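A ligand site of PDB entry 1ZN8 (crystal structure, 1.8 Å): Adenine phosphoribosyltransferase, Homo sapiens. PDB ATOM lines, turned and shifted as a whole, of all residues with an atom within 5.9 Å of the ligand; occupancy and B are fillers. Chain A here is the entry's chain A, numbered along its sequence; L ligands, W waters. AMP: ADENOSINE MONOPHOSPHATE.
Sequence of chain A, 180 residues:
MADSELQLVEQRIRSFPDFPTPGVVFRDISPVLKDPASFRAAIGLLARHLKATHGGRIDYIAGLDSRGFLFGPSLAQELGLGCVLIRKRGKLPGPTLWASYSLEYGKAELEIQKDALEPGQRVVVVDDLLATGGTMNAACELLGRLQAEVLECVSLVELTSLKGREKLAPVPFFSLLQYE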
ATOM      1  N   PHE A  19      28.667  30.290   0.760  1.00  0.00           N
ATOM      2  CA  PHE A  19      27.896  31.270   1.513  1.00  0.00           C
ATOM      3  C   PHE A  19      28.045  30.957   2.994  1.00  0.00           C
ATOM      4  O   PHE A  19      27.908  29.821   3.388  1.00  0.00           O
ATOM      5  CB  PHE A  19      26.440  31.246   1.064  1.00  0.00           C
ATOM      6  CG  PHE A  19      25.589  32.227   1.797  1.00  0.00           C
ATOM      7  CD1 PHE A  19      25.479  33.534   1.353  1.00  0.00           C
ATOM      8  CD2 PHE A  19      24.985  31.875   2.973  1.00  0.00           C
ATOM      9  CE1 PHE A  19      24.750  34.475   2.073  1.00  0.00           C
ATOM     10  CE2 PHE A  19      24.230  32.781   3.706  1.00  0.00           C
ATOM     11  CZ  PHE A  19      24.120  34.088   3.262  1.00  0.00           C
ATOM     12  N   VAL A  24      32.620  28.030   3.098  1.00  0.00           N
ATOM     13  CA  VAL A  24      31.488  27.507   3.856  1.00  0.00           C
ATOM     14  C   VAL A  24      30.463  26.938   2.880  1.00  0.00           C
ATOM     15  O   VAL A  24      30.104  27.643   1.955  1.00  0.00           O
ATOM     16  CB  VAL A  24      30.758  28.610   4.663  1.00  0.00           C
ATOM     17  CG1 VAL A  24      29.604  28.031   5.495  1.00  0.00           C
ATOM     18  CG2 VAL A  24      31.682  29.332   5.615  1.00  0.00           C
ATOM     19  N   VAL A  25      30.009  25.691   3.054  1.00  0.00           N
ATOM     20  CA  VAL A  25      28.853  25.149   2.312  1.00  0.00           C
ATOM     21  C   VAL A  25      27.607  25.287   3.196  1.00  0.00           C
ATOM     22  O   VAL A  25      27.460  24.579   4.190  1.00  0.00           O
ATOM     23  CB  VAL A  25      29.034  23.685   1.864  1.00  0.00           C
ATOM     24  CG1 VAL A  25      27.774  23.151   1.171  1.00  0.00           C
ATOM     25  CG2 VAL A  25      30.204  23.520   0.913  1.00  0.00           C
ATOM     26  N   PHE A  26      26.776  26.267   2.894  1.00  0.00           N
ATOM     27  CA  PHE A  26      25.616  26.511   3.658  1.00  0.00           C
ATOM     28  C   PHE A  26      24.543  25.444   3.407  1.00  0.00           C
ATOM     29  O   PHE A  26      24.245  25.109   2.272  1.00  0.00           O
ATOM     30  CB  PHE A  26      25.122  27.912   3.294  1.00  0.00           C
ATOM     31  CG  PHE A  26      24.064  28.435   4.260  1.00  0.00           C
ATOM     32  CD1 PHE A  26      24.410  29.197   5.345  1.00  0.00           C
ATOM     33  CD2 PHE A  26      22.721  28.186   4.019  1.00  0.00           C
ATOM     34  CE1 PHE A  26      23.394  29.698   6.209  1.00  0.00           C
ATOM     35  CE2 PHE A  26      21.700  28.681   4.895  1.00  0.00           C
ATOM     36  CZ  PHE A  26      22.062  29.411   5.954  1.00  0.00           C
ATOM     37  N   ARG A  27      24.012  24.897   4.513  1.00  0.00           N
ATOM     38  CA  ARG A  27      22.928  23.946   4.510  1.00  0.00           C
ATOM     39  C   ARG A  27      21.693  24.702   4.926  1.00  0.00           C
ATOM     40  O   ARG A  27      21.589  25.206   6.074  1.00  0.00           O
ATOM     41  CB  ARG A  27      23.214  22.790   5.469  1.00  0.00           C
ATOM     42  CG  ARG A  27      24.606  22.220   5.313  1.00  0.00           C
ATOM     43  CD  ARG A  27      24.802  21.574   3.984  1.00  0.00           C
ATOM     44  NE  ARG A  27      26.161  21.026   3.934  1.00  0.00           N
ATOM     45  CZ  ARG A  27      26.613  20.171   3.016  1.00  0.00           C
ATOM     46  NH1 ARG A  27      25.847  19.714   2.046  1.00  0.00           N
ATOM     47  NH2 ARG A  27      27.854  19.747   3.092  1.00  0.00           N
ATOM     48  N   ASP A  28      20.784  24.846   3.970  1.00  0.00           N
ATOM     49  CA  ASP A  28      19.539  25.637   4.159  1.00  0.00           C
ATOM     50  C   ASP A  28      18.393  24.675   4.455  1.00  0.00           C
ATOM     51  O   ASP A  28      18.000  23.855   3.602  1.00  0.00           O
ATOM     52  CB  ASP A  28      19.273  26.476   2.873  1.00  0.00           C
ATOM     53  CG  ASP A  28      18.025  27.332   2.947  1.00  0.00           C
ATOM     54  OD1 ASP A  28      17.560  27.630   4.038  1.00  0.00           O
ATOM     55  OD2 ASP A  28      17.556  27.740   1.883  1.00  0.00           O
ATOM     56  N   ASP A  65      18.186  31.007  19.263  1.00  0.00           N
ATOM     57  CA  ASP A  65      17.963  32.127  18.341  1.00  0.00           C
ATOM     58  C   ASP A  65      18.925  32.060  17.186  1.00  0.00           C
ATOM     59  O   ASP A  65      20.148  31.967  17.425  1.00  0.00           O
ATOM     60  CB  ASP A  65      18.177  33.406  19.191  1.00  0.00           C
ATOM     61  CG  ASP A  65      17.721  34.688  18.547  1.00  0.00           C
ATOM     62  OD1 ASP A  65      17.665  35.708  19.279  1.00  0.00           O
ATOM     63  OD2 ASP A  65      17.384  34.709  17.346  1.00  0.00           O
ATOM     64  N   ARG A  67      17.294  30.264  14.201  1.00  0.00           N
ATOM     65  CA  ARG A  67      16.734  29.042  13.515  1.00  0.00           C
ATOM     66  C   ARG A  67      16.303  27.887  14.404  1.00  0.00           C
ATOM     67  O   ARG A  67      15.454  27.081  14.027  1.00  0.00           O
ATOM     68  CB  ARG A  67      17.645  28.570  12.411  1.00  0.00           C
ATOM     69  CG  ARG A  67      17.609  29.490  11.239  1.00  0.00           C
ATOM     70  CD  ARG A  67      18.545  29.060  10.167  1.00  0.00           C
ATOM     71  NE  ARG A  67      19.818  29.774  10.253  1.00  0.00           N
ATOM     72  CZ  ARG A  67      21.015  29.263   9.966  1.00  0.00           C
ATOM     73  NH1 ARG A  67      21.157  27.996   9.631  1.00  0.00           N
ATOM     74  NH2 ARG A  67      22.090  30.024  10.059  1.00  0.00           N
ATOM     75  N   TYR A 101      31.106  33.572  22.591  1.00  0.00           N
ATOM     76  CA  TYR A 101      31.624  32.444  21.851  1.00  0.00           C
ATOM     77  C   TYR A 101      32.121  33.026  20.541  1.00  0.00           C
ATOM     78  O   TYR A 101      31.794  34.163  20.151  1.00  0.00           O
ATOM     79  CB  TYR A 101      30.550  31.335  21.630  1.00  0.00           C
ATOM     80  CG  TYR A 101      29.400  31.767  20.797  1.00  0.00           C
ATOM     81  CD1 TYR A 101      28.397  32.557  21.347  1.00  0.00           C
ATOM     82  CD2 TYR A 101      29.343  31.464  19.449  1.00  0.00           C
ATOM     83  CE1 TYR A 101      27.306  33.015  20.572  1.00  0.00           C
ATOM     84  CE2 TYR A 101      28.238  31.909  18.635  1.00  0.00           C
ATOM     85  CZ  TYR A 101      27.241  32.688  19.243  1.00  0.00           C
ATOM     86  OH  TYR A 101      26.203  33.181  18.492  1.00  0.00           O
ATOM     87  N   SER A 102      32.953  32.246  19.881  1.00  0.00           N
ATOM     88  CA  SER A 102      33.544  32.659  18.634  1.00  0.00           C
ATOM     89  C   SER A 102      32.528  32.314  17.542  1.00  0.00           C
ATOM     90  O   SER A 102      32.061  31.151  17.417  1.00  0.00           O
ATOM     91  CB  SER A 102      34.883  31.947  18.426  1.00  0.00           C
ATOM     92  OG  SER A 102      35.369  32.093  17.093  1.00  0.00           O
ATOM     93  N   LEU A 103      32.181  33.323  16.746  1.00  0.00           N
ATOM     94  CA  LEU A 103      31.352  33.101  15.579  1.00  0.00           C
ATOM     95  C   LEU A 103      31.996  33.813  14.402  1.00  0.00           C
ATOM     96  O   LEU A 103      32.209  35.025  14.466  1.00  0.00           O
ATOM     97  CB  LEU A 103      29.931  33.600  15.824  1.00  0.00           C
ATOM     98  CG  LEU A 103      28.801  32.995  14.952  1.00  0.00           C
ATOM     99  CD1 LEU A 103      28.724  33.729  13.643  1.00  0.00           C
ATOM    100  CD2 LEU A 103      28.933  31.479  14.696  1.00  0.00           C
ATOM    101  N   ASP A 127      18.839  23.280  17.845  1.00  0.00           N
ATOM    102  CA  ASP A 127      19.142  24.267  16.814  1.00  0.00           C
ATOM    103  C   ASP A 127      19.064  23.543  15.480  1.00  0.00           C
ATOM    104  O   ASP A 127      18.995  22.287  15.428  1.00  0.00           O
ATOM    105  CB  ASP A 127      20.529  24.806  17.013  1.00  0.00           C
ATOM    106  CG  ASP A 127      20.736  26.229  16.459  1.00  0.00           C
ATOM    107  OD1 ASP A 127      19.841  26.808  15.810  1.00  0.00           O
ATOM    108  OD2 ASP A 127      21.859  26.757  16.692  1.00  0.00           O
ATOM    109  N   ASP A 128      19.099  24.303  14.391  1.00  0.00           N
ATOM    110  CA  ASP A 128      18.980  23.635  13.108  1.00  0.00           C
ATOM    111  C   ASP A 128      20.172  22.784  12.770  1.00  0.00           C
ATOM    112  O   ASP A 128      20.033  21.722  12.182  1.00  0.00           O
ATOM    113  CB  ASP A 128      18.589  24.565  11.969  1.00  0.00           C
ATOM    114  CG  ASP A 128      19.624  25.628  11.654  1.00  0.00           C
ATOM    115  OD1 ASP A 128      19.607  26.125  10.505  1.00  0.00           O
ATOM    116  OD2 ASP A 128      20.450  25.984  12.542  1.00  0.00           O
ATOM    117  N   LEU A 129      21.362  23.296  13.094  1.00  0.00           N
ATOM    118  CA  LEU A 129      22.582  22.714  12.594  1.00  0.00           C
ATOM    119  C   LEU A 129      23.693  22.886  13.655  1.00  0.00           C
ATOM    120  O   LEU A 129      23.827  23.992  14.246  1.00  0.00           O
ATOM    121  CB  LEU A 129      22.909  23.445  11.286  1.00  0.00           C
ATOM    122  CG  LEU A 129      24.202  23.615  10.464  1.00  0.00           C
ATOM    123  CD1 LEU A 129      25.503  23.574  11.184  1.00  0.00           C
ATOM    124  CD2 LEU A 129      24.177  22.868   9.229  1.00  0.00           C
ATOM    125  N   LEU A 130      24.490  21.826  13.816  1.00  0.00           N
ATOM    126  CA  LEU A 130      25.729  21.828  14.631  1.00  0.00           C
ATOM    127  C   LEU A 130      26.916  21.893  13.699  1.00  0.00           C
ATOM    128  O   LEU A 130      27.045  21.065  12.838  1.00  0.00           O
ATOM    129  CB  LEU A 130      25.864  20.563  15.483  1.00  0.00           C
ATOM    130  CG  LEU A 130      27.036  20.545  16.453  1.00  0.00           C
ATOM    131  CD1 LEU A 130      26.764  21.337  17.690  1.00  0.00           C
ATOM    132  CD2 LEU A 130      27.407  19.174  16.834  1.00  0.00           C
ATOM    133  N   ALA A 131      27.768  22.886  13.887  1.00  0.00           N
ATOM    134  CA  ALA A 131      29.004  22.989  13.099  1.00  0.00           C
ATOM    135  C   ALA A 131      30.103  22.889  14.114  1.00  0.00           C
ATOM    136  O   ALA A 131      30.344  21.785  14.625  1.00  0.00           O
ATOM    137  CB  ALA A 131      28.984  24.270  12.326  1.00  0.00           C
ATOM    138  N   THR A 132      30.733  23.989  14.524  1.00  0.00           N
ATOM    139  CA  THR A 132      31.801  23.922  15.532  1.00  0.00           C
ATOM    140  C   THR A 132      31.325  23.588  16.940  1.00  0.00           C
ATOM    141  O   THR A 132      32.130  23.129  17.769  1.00  0.00           O
ATOM    142  CB  THR A 132      32.675  25.200  15.657  1.00  0.00           C
ATOM    143  OG1 THR A 132      31.928  26.273  16.236  1.00  0.00           O
ATOM    144  CG2 THR A 132      33.231  25.646  14.316  1.00  0.00           C
ATOM    145  N   GLY A 133      30.023  23.797  17.192  1.00  0.00           N
ATOM    146  CA  GLY A 133      29.426  23.662  18.522  1.00  0.00           C
ATOM    147  C   GLY A 133      29.577  24.878  19.439  1.00  0.00           C
ATOM    148  O   GLY A 133      29.162  24.840  20.594  1.00  0.00           O
ATOM    149  N   GLY A 134      30.140  25.978  18.962  1.00  0.00           N
ATOM    150  CA  GLY A 134      30.247  27.175  19.790  1.00  0.00           C
ATOM    151  C   GLY A 134      28.909  27.695  20.289  1.00  0.00           C
ATOM    152  O   GLY A 134      28.781  28.052  21.440  1.00  0.00           O
ATOM    153  N   THR A 135      27.895  27.715  19.429  1.00  0.00           N
ATOM    154  CA  THR A 135      26.570  28.226  19.793  1.00  0.00           C
ATOM    155  C   THR A 135      25.943  27.297  20.854  1.00  0.00           C
ATOM    156  O   THR A 135      25.493  27.724  21.922  1.00  0.00           O
ATOM    157  CB  THR A 135      25.725  28.350  18.516  1.00  0.00           C
ATOM    158  OG1 THR A 135      26.446  29.152  17.573  1.00  0.00           O
ATOM    159  CG2 THR A 135      24.421  29.040  18.789  1.00  0.00           C
ATOM    160  N   MET A 136      25.933  25.998  20.560  1.00  0.00           N
ATOM    161  CA  MET A 136      25.380  25.031  21.484  1.00  0.00           C
ATOM    162  C   MET A 136      26.136  24.981  22.790  1.00  0.00           C
ATOM    163  O   MET A 136      25.536  24.742  23.810  1.00  0.00           O
ATOM    164  CB  MET A 136      25.323  23.617  20.898  1.00  0.00           C
ATOM    165  CG  MET A 136      23.929  23.121  20.640  1.00  0.00           C
ATOM    166  SD  MET A 136      23.804  21.948  19.268  1.00  0.00           S
ATOM    167  CE  MET A 136      22.198  22.318  18.678  1.00  0.00           C
ATOM    168  N   LEU A 159      27.747  18.867  10.897  1.00  0.00           N
ATOM    169  CA  LEU A 159      28.896  18.870   9.985  1.00  0.00           C
ATOM    170  C   LEU A 159      30.039  18.195  10.712  1.00  0.00           C
ATOM    171  O   LEU A 159      30.646  18.789  11.598  1.00  0.00           O
ATOM    172  CB  LEU A 159      29.239  20.327   9.623  1.00  0.00           C
ATOM    173  CG  LEU A 159      28.348  21.080   8.608  1.00  0.00           C
ATOM    174  CD1 LEU A 159      27.086  20.460   8.086  1.00  0.00           C
ATOM    175  CD2 LEU A 159      28.317  22.542   8.894  1.00  0.00           C
ATOM    176  N   LEU A 162      33.821  19.171  11.774  1.00  0.00           N
ATOM    177  CA  LEU A 162      34.022  20.315  12.602  1.00  0.00           C
ATOM    178  C   LEU A 162      34.025  19.995  14.106  1.00  0.00           C
ATOM    179  O   LEU A 162      34.255  20.891  14.912  1.00  0.00           O
ATOM    180  CB  LEU A 162      32.966  21.323  12.251  1.00  0.00           C
ATOM    181  CG  LEU A 162      33.280  22.452  11.287  1.00  0.00           C
ATOM    182  CD1 LEU A 162      34.297  22.300  10.236  1.00  0.00           C
ATOM    183  CD2 LEU A 162      31.992  23.059  10.766  1.00  0.00           C
HETATM  184  P   AMP L   1      28.521  26.669  15.427  1.00  0.00           P
HETATM  185  O1P AMP L   1      28.314  27.634  16.600  1.00  0.00           O
HETATM  186  O2P AMP L   1      27.976  25.305  15.663  1.00  0.00           O
HETATM  187  O3P AMP L   1      29.828  26.736  14.681  1.00  0.00           O
HETATM  188  O5' AMP L   1      27.562  27.346  14.360  1.00  0.00           O
HETATM  189  C5' AMP L   1      26.200  26.951  14.355  1.00  0.00           C
HETATM  190  C4' AMP L   1      25.347  28.170  14.083  1.00  0.00           C
HETATM  191  O4' AMP L   1      25.741  28.778  12.840  1.00  0.00           O
HETATM  192  C3' AMP L   1      23.985  27.596  13.973  1.00  0.00           C
HETATM  193  O3' AMP L   1      23.103  28.565  14.548  1.00  0.00           O
HETATM  194  C2' AMP L   1      23.785  27.350  12.500  1.00  0.00           C
HETATM  195  O2' AMP L   1      22.443  27.751  12.160  1.00  0.00           O
HETATM  196  C1' AMP L   1      24.854  28.274  11.849  1.00  0.00           C
HETATM  197  N9  AMP L   1      25.661  27.565  10.853  1.00  0.00           N
HETATM  198  C8  AMP L   1      26.969  27.282  10.953  1.00  0.00           C
HETATM  199  N7  AMP L   1      27.433  26.656   9.845  1.00  0.00           N
HETATM  200  C5  AMP L   1      26.374  26.548   9.003  1.00  0.00           C
HETATM  201  C6  AMP L   1      26.179  26.001   7.675  1.00  0.00           C
HETATM  202  N6  AMP L   1      27.186  25.437   7.015  1.00  0.00           N
HETATM  203  N1  AMP L   1      24.940  26.108   7.154  1.00  0.00           N
HETATM  204  C2  AMP L   1      23.884  26.678   7.844  1.00  0.00           C
HETATM  205  N3  AMP L   1      23.978  27.224   9.082  1.00  0.00           N
HETATM  206  C4  AMP L   1      25.199  27.188   9.672  1.00  0.00           C
HETATM  207  O   HOH W   1      26.435  25.040  17.853  1.00  0.00           O
HETATM  208  O   HOH W   2      21.931  29.721  16.662  1.00  0.00           O
HETATM  209  O   HOH W   3      30.016  26.534   9.469  1.00  0.00           O
HETATM  210  O   HOH W   4      30.269  29.342  16.855  1.00  0.00           O
HETATM  211  O   HOH W   5      30.506  27.956  12.255  1.00  0.00           O
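O1P of the ligand is in hydrogen-bond range of N of Thr 135 (2.9 Å). O1P of the ligand lies within hydrogen-bond range of OG1 of Thr 135 (2.6 Å). The backbone NH of Thr 132 lies within hydrogen-bond range of an oxygen (O3P) of the ligand (2.9 Å). The side-chain hydroxyl (OG1) of Thr 132 lies within hydrogen-bond range of an oxygen (O3P) of the ligand (2.7 Å). OD2 of Asp 128 sits at hydrogen-bond distance from O2' of the ligand, at 2.7 Å. An oxygen (O2') of the ligand sits at hydrogen-bond distance from the guanidinium group (NH1) of Arg 67, 2.8 Å away. The backbone carbonyl oxygen (O) of Val 25 lies within hydrogen-bond range of a nitrogen (N6) of the ligand (3.0 Å). N of Gly 133 lies within hydrogen-bond range of O2P of the ligand, 3.0 Å away. O2P of the ligand is in hydrogen-bond range of N of Ala 131 (3.0 Å). The backbone NH (N) of Arg 27 sits at hydrogen-bond distance from a nitrogen (N1) of the ligand. An oxygen (O3') of the ligand is in hydrogen-bond range of the side-chain carboxylate of Asp 127. The backbone NH of Gly 134 lies within hydrogen-bond range of an oxygen (O1P) of the ligand.
The backbone NH (N) of Gly 134 sits at hydrogen-bond distance from the side-chain hydroxyl (OG1) of Thr 132. NH1 of Arg 67 is in salt-bridge range of OD1 of Asp 128. The backbone NH of Leu 159 is in hydrogen-bond range of the backbone carbonyl oxygen of Leu 130 (3.0 Å). O of Val 24 sits at hydrogen-bond distance from N of Phe 19, at 3.2 Å.
Val 24 touches the ligand. Phe 26 touches the ligand. O of Leu 129 touches C3' of the ligand (3.6 Å). CD2 of Leu 159 touches N6 of the ligand, at 3.6 Å. Hydrophobic or aromatic side chains that line the ligand: Val 24, Phe 26, Leu 129, Ala 131 and Leu 159. Within 4 Å of the ligand: Val 24, Val 25, Phe 26, Arg 27, Arg 67, Asp 127, Asp 128, Leu 129, Ala 131, Thr 132, Gly 133, Gly 134, Thr 135 and Leu 159.
Water W4 lies within hydrogen-bond range of the backbone carbonyl oxygen of Ser 102 (2.6 Å) and an oxygen (O1P) of the ligand (2.6 Å). Water W2 lies within hydrogen-bond range of O3' of the ligand (2.7 Å), OD2 of Asp 127 (3.0 Å) and O of Asp 65 (3.0 Å). Water W1 lies within hydrogen-bond range of an oxygen (O2P) of the ligand (2.7 Å), the backbone NH (N) of Met 136 (2.9 Å) and the backbone NH (N) of Thr 135 (3.4 Å).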
